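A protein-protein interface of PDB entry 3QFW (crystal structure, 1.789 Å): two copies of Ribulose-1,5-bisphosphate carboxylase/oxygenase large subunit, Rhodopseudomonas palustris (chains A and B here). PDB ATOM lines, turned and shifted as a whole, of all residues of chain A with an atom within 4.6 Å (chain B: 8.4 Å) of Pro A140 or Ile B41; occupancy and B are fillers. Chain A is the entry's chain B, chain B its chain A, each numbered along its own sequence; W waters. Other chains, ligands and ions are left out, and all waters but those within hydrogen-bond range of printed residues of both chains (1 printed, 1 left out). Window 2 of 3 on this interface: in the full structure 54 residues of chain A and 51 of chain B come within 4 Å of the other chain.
The side-chain amide oxygen (OE1) of Gln A141 sits close to the backbone carbonyl oxygen (O) of Ser B33, 3.3 Å away.
The side-chain amino group (NZ) of Lys A139 is in salt-bridge range of the side-chain carboxylate (OE2) of Glu B35 (3.1 Å).
The backbone carbonyl oxygen of Val B34 sits at hydrogen-bond distance from the side-chain sulfur of Cys B36.
The side-chain hydroxyl (OG) of Ser B33 sits at hydrogen-bond distance from the backbone carbonyl oxygen (O) of Ile B50 (2.5 Å).
The backbone NH of Glu B35 sits at hydrogen-bond distance from the backbone carbonyl oxygen of Ile B30 (2.9 Å).
The backbone NH (N) of Gly B52 sits at hydrogen-bond distance from the side-chain hydroxyl (OG) of Ser B33.
Lys A139 touches Val B34.
Cys B36 touches Lys A139.
CB of Pro A140 touches CG1 of Val B34 (3.9 Å).
Cys B36 touches Pro A140 (SG to CB, 3.7 Å).
CG1 of Ile B41 touches CG of Pro A140, 3.9 Å away.
Gly A142 touches Ile B50.
Of the printed residues of chain B, Lys A139 touches Val B34, Glu B35 and Cys B36.
Printed residues of chain B within 4 Å of Pro A140: Val B34 (3.9 Å), Cys B36 (3.7 Å) and Ile B41 (3.9 Å).
Ile B30 touches none of the printed residues of chain A.
Of the printed residues of chain A, Ser B33 touches Gln A141 (3.3 Å).
Printed residues of chain A within 4 Å of Val B34: Lys A139 and Pro A140.
Of the printed residues of chain A, Glu B35 touches Lys A139.
Printed residues of chain A within 4 Å of Cys B36: Lys A139 (3.3 Å) and Pro A140 (3.7 Å).
Glu B39 touches none of the printed residues of chain A.
The nearest residue of chain B that does not touch Pro A140 is Ala B40 (4.3 Å).
Printed residues of chain B that touch a printed residue of chain A: Ser B33, Val B34, Glu B35, Cys B36, Ile B41 and Ile B50.
Hydrophobic or aromatic side chains of chain B that line the printed part of chain A: Val B34, Ile B41 and Ile B50.
No position is printed for both chains.
Of the 8 pairs that touch across the chains among the printed residues, none has its exchanged pair printed and touching as well.
Water W1 bridges O of Ser B33 (2.7 Å) and OE1 of Gln A141 (3.2 Å).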
ATOM      1  N   LYS A 139      11.600  -7.177 -17.975  1.00  0.00           N
ATOM      2  CA  LYS A 139      12.669  -7.175 -16.989  1.00  0.00           C
ATOM      3  C   LYS A 139      12.081  -6.570 -15.730  1.00  0.00           C
ATOM      4  O   LYS A 139      11.146  -5.763 -15.815  1.00  0.00           O
ATOM      5  CB  LYS A 139      13.820  -6.293 -17.473  1.00  0.00           C
ATOM      6  CG  LYS A 139      14.354  -6.658 -18.844  1.00  0.00           C
ATOM      7  CD  LYS A 139      15.494  -5.745 -19.259  1.00  0.00           C
ATOM      8  CE  LYS A 139      16.193  -6.283 -20.501  1.00  0.00           C
ATOM      9  NZ  LYS A 139      17.318  -5.411 -20.951  1.00  0.00           N
ATOM     10  N   PRO A 140      12.634  -6.917 -14.555  1.00  0.00           N
ATOM     11  CA  PRO A 140      13.780  -7.807 -14.308  1.00  0.00           C
ATOM     12  C   PRO A 140      13.399  -9.277 -14.092  1.00  0.00           C
ATOM     13  O   PRO A 140      12.290  -9.570 -13.656  1.00  0.00           O
ATOM     14  CB  PRO A 140      14.372  -7.237 -13.016  1.00  0.00           C
ATOM     15  CG  PRO A 140      13.175  -6.710 -12.275  1.00  0.00           C
ATOM     16  CD  PRO A 140      12.207  -6.211 -13.331  1.00  0.00           C
ATOM     17  N   GLN A 141      14.331 -10.187 -14.375  1.00  0.00           N
ATOM     18  CA  GLN A 141      14.064 -11.629 -14.306  1.00  0.00           C
ATOM     19  C   GLN A 141      13.792 -12.211 -12.902  1.00  0.00           C
ATOM     20  O   GLN A 141      13.510 -13.397 -12.768  1.00  0.00           O
ATOM     21  CB  GLN A 141      15.189 -12.433 -14.985  1.00  0.00           C
ATOM     22  CG  GLN A 141      16.595 -12.140 -14.486  1.00  0.00           C
ATOM     23  CD  GLN A 141      17.592 -13.240 -14.844  1.00  0.00           C
ATOM     24  OE1 GLN A 141      18.611 -12.989 -15.492  1.00  0.00           O
ATOM     25  NE2 GLN A 141      17.307 -14.465 -14.410  1.00  0.00           N
ATOM     26  N   GLY A 142      13.879 -11.400 -11.863  1.00  0.00           N
ATOM     27  CA  GLY A 142      13.536 -11.895 -10.538  1.00  0.00           C
ATOM     28  C   GLY A 142      12.039 -12.088 -10.321  1.00  0.00           C
ATOM     29  O   GLY A 142      11.622 -12.739  -9.359  1.00  0.00           O
ATOM     30  N   LEU A 143      11.236 -11.538 -11.229  1.00  0.00           N
ATOM     31  CA  LEU A 143       9.783 -11.425 -11.057  1.00  0.00           C
ATOM     32  C   LEU A 143       8.991 -12.716 -11.263  1.00  0.00           C
ATOM     33  O   LEU A 143       9.402 -13.601 -12.007  1.00  0.00           O
ATOM     34  CB  LEU A 143       9.228 -10.350 -12.004  1.00  0.00           C
ATOM     35  CG  LEU A 143       9.574  -8.901 -11.673  1.00  0.00           C
ATOM     36  CD1 LEU A 143       9.211  -7.970 -12.828  1.00  0.00           C
ATOM     37  CD2 LEU A 143       8.874  -8.483 -10.381  1.00  0.00           C
ATOM     38  N   LEU A 148       5.441 -10.254 -14.259  1.00  0.00           N
ATOM     39  CA  LEU A 148       5.883 -10.139 -15.645  1.00  0.00           C
ATOM     40  C   LEU A 148       4.673  -9.893 -16.540  1.00  0.00           C
ATOM     41  O   LEU A 148       4.711  -9.042 -17.433  1.00  0.00           O
ATOM     42  CB  LEU A 148       6.621 -11.414 -16.090  1.00  0.00           C
ATOM     43  CG  LEU A 148       7.939 -11.765 -15.387  1.00  0.00           C
ATOM     44  CD1 LEU A 148       8.436 -13.136 -15.823  1.00  0.00           C
ATOM     45  CD2 LEU A 148       8.993 -10.698 -15.662  1.00  0.00           C
ATOM     46  N   ILE B  30      25.346  -5.565 -13.288  1.00  0.00           N
ATOM     47  CA  ILE B  30      23.999  -5.387 -13.838  1.00  0.00           C
ATOM     48  C   ILE B  30      23.794  -6.157 -15.143  1.00  0.00           C
ATOM     49  O   ILE B  30      22.811  -6.885 -15.295  1.00  0.00           O
ATOM     50  CB  ILE B  30      23.678  -3.894 -14.098  1.00  0.00           C
ATOM     51  CG1 ILE B  30      23.632  -3.117 -12.783  1.00  0.00           C
ATOM     52  CG2 ILE B  30      22.355  -3.751 -14.816  1.00  0.00           C
ATOM     53  CD1 ILE B  30      22.581  -3.621 -11.838  1.00  0.00           C
ATOM     54  N   SER B  33      23.075  -9.643 -14.872  1.00  0.00           N
ATOM     55  CA  SER B  33      22.007  -9.871 -13.923  1.00  0.00           C
ATOM     56  C   SER B  33      20.672  -9.450 -14.511  1.00  0.00           C
ATOM     57  O   SER B  33      20.121 -10.102 -15.399  1.00  0.00           O
ATOM     58  CB  SER B  33      22.269  -9.079 -12.638  1.00  0.00           C
ATOM     59  OG  SER B  33      21.455  -9.573 -11.603  1.00  0.00           O
ATOM     60  N   VAL B  34      20.168  -8.339 -14.001  1.00  0.00           N
ATOM     61  CA  VAL B  34      18.842  -7.869 -14.351  1.00  0.00           C
ATOM     62  C   VAL B  34      18.844  -7.083 -15.651  1.00  0.00           C
ATOM     63  O   VAL B  34      17.813  -6.984 -16.312  1.00  0.00           O
ATOM     64  CB  VAL B  34      18.289  -6.995 -13.234  1.00  0.00           C
ATOM     65  CG1 VAL B  34      18.041  -7.847 -12.002  1.00  0.00           C
ATOM     66  CG2 VAL B  34      19.272  -5.873 -12.929  1.00  0.00           C
ATOM     67  N   GLU B  35      19.993  -6.513 -15.995  1.00  0.00           N
ATOM     68  CA  GLU B  35      20.145  -5.821 -17.251  1.00  0.00           C
ATOM     69  C   GLU B  35      19.084  -4.705 -17.292  1.00  0.00           C
ATOM     70  O   GLU B  35      18.453  -4.457 -18.318  1.00  0.00           O
ATOM     71  CB  GLU B  35      19.973  -6.824 -18.393  1.00  0.00           C
ATOM     72  CG  GLU B  35      20.266  -6.287 -19.786  1.00  0.00           C
ATOM     73  CD  GLU B  35      19.971  -7.316 -20.862  1.00  0.00           C
ATOM     74  OE1 GLU B  35      19.953  -8.523 -20.532  1.00  0.00           O
ATOM     75  OE2 GLU B  35      19.745  -6.922 -22.026  1.00  0.00           O
ATOM     76  N   CYS B  36      18.902  -4.064 -16.138  1.00  0.00           N
ATOM     77  CA  CYS B  36      17.923  -3.000 -15.914  1.00  0.00           C
ATOM     78  C   CYS B  36      18.635  -1.797 -15.333  1.00  0.00           C
ATOM     79  O   CYS B  36      19.636  -1.949 -14.642  1.00  0.00           O
ATOM     80  CB  CYS B  36      16.921  -3.423 -14.830  1.00  0.00           C
ATOM     81  SG  CYS B  36      15.696  -4.644 -15.249  1.00  0.00           S
ATOM     82  N   PRO B  37      18.104  -0.591 -15.573  1.00  0.00           N
ATOM     83  CA  PRO B  37      18.480   0.475 -14.644  1.00  0.00           C
ATOM     84  C   PRO B  37      17.843   0.149 -13.296  1.00  0.00           C
ATOM     85  O   PRO B  37      16.790  -0.488 -13.273  1.00  0.00           O
ATOM     86  CB  PRO B  37      17.818   1.715 -15.252  1.00  0.00           C
ATOM     87  CG  PRO B  37      17.671   1.388 -16.707  1.00  0.00           C
ATOM     88  CD  PRO B  37      17.374  -0.082 -16.746  1.00  0.00           C
ATOM     89  N   LEU B  38      18.465   0.550 -12.193  1.00  0.00           N
ATOM     90  CA  LEU B  38      17.883   0.276 -10.881  1.00  0.00           C
ATOM     91  C   LEU B  38      16.494   0.923 -10.730  1.00  0.00           C
ATOM     92  O   LEU B  38      15.618   0.379 -10.054  1.00  0.00           O
ATOM     93  CB  LEU B  38      18.841   0.694  -9.759  1.00  0.00           C
ATOM     94  CG  LEU B  38      20.053  -0.234  -9.571  1.00  0.00           C
ATOM     95  CD1 LEU B  38      21.087   0.346  -8.599  1.00  0.00           C
ATOM     96  CD2 LEU B  38      19.612  -1.622  -9.113  1.00  0.00           C
ATOM     97  N   GLU B  39      16.290   2.064 -11.384  1.00  0.00           N
ATOM     98  CA  GLU B  39      14.986   2.734 -11.365  1.00  0.00           C
ATOM     99  C   GLU B  39      13.882   1.844 -11.935  1.00  0.00           C
ATOM    100  O   GLU B  39      12.703   2.027 -11.627  1.00  0.00           O
ATOM    101  CB  GLU B  39      15.034   4.071 -12.118  1.00  0.00           C
ATOM    102  CG  GLU B  39      13.645   4.658 -12.423  1.00  0.00           C
ATOM    103  CD  GLU B  39      13.669   6.138 -12.786  1.00  0.00           C
ATOM    104  OE1 GLU B  39      12.967   6.921 -12.112  1.00  0.00           O
ATOM    105  OE2 GLU B  39      14.371   6.518 -13.749  1.00  0.00           O
ATOM    106  N   ALA B  40      14.266   0.868 -12.750  1.00  0.00           N
ATOM    107  CA  ALA B  40      13.293  -0.007 -13.395  1.00  0.00           C
ATOM    108  C   ALA B  40      12.857  -1.150 -12.484  1.00  0.00           C
ATOM    109  O   ALA B  40      12.007  -1.961 -12.854  1.00  0.00           O
ATOM    110  CB  ALA B  40      13.851  -0.549 -14.711  1.00  0.00           C
ATOM    111  N   ILE B  41      13.437  -1.222 -11.293  1.00  0.00           N
ATOM    112  CA  ILE B  41      13.083  -2.280 -10.354  1.00  0.00           C
ATOM    113  C   ILE B  41      12.334  -1.720  -9.149  1.00  0.00           C
ATOM    114  O   ILE B  41      11.181  -2.078  -8.906  1.00  0.00           O
ATOM    115  CB  ILE B  41      14.319  -3.057  -9.867  1.00  0.00           C
ATOM    116  CG1 ILE B  41      15.118  -3.606 -11.051  1.00  0.00           C
ATOM    117  CG2 ILE B  41      13.910  -4.198  -8.939  1.00  0.00           C
ATOM    118  CD1 ILE B  41      16.187  -4.607 -10.635  1.00  0.00           C
ATOM    119  N   ILE B  50      18.780 -10.539  -6.606  1.00  0.00           N
ATOM    120  CA  ILE B  50      19.022 -10.929  -7.991  1.00  0.00           C
ATOM    121  C   ILE B  50      20.102 -10.088  -8.659  1.00  0.00           C
ATOM    122  O   ILE B  50      20.960 -10.623  -9.355  1.00  0.00           O
ATOM    123  CB  ILE B  50      17.728 -10.827  -8.821  1.00  0.00           C
ATOM    124  CG1 ILE B  50      16.604 -11.601  -8.134  1.00  0.00           C
ATOM    125  CG2 ILE B  50      17.945 -11.321 -10.245  1.00  0.00           C
ATOM    126  CD1 ILE B  50      17.011 -12.967  -7.689  1.00  0.00           C
ATOM    127  N   VAL B  51      20.056  -8.774  -8.464  1.00  0.00           N
ATOM    128  CA  VAL B  51      21.117  -7.917  -8.981  1.00  0.00           C
ATOM    129  C   VAL B  51      22.477  -8.524  -8.619  1.00  0.00           C
ATOM    130  O   VAL B  51      22.668  -9.012  -7.512  1.00  0.00           O
ATOM    131  CB  VAL B  51      21.015  -6.484  -8.427  1.00  0.00           C
ATOM    132  CG1 VAL B  51      22.163  -5.636  -8.941  1.00  0.00           C
ATOM    133  CG2 VAL B  51      19.672  -5.858  -8.806  1.00  0.00           C
ATOM    134  N   GLY B  52      23.413  -8.512  -9.561  1.00  0.00           N
ATOM    135  CA  GLY B  52      24.740  -9.045  -9.304  1.00  0.00           C
ATOM    136  C   GLY B  52      25.483  -8.161  -8.324  1.00  0.00           C
ATOM    137  O   GLY B  52      25.312  -6.933  -8.317  1.00  0.00           O
HETATM  138  O   HOH W   1      19.667 -11.077 -17.872  1.00  0.00           O
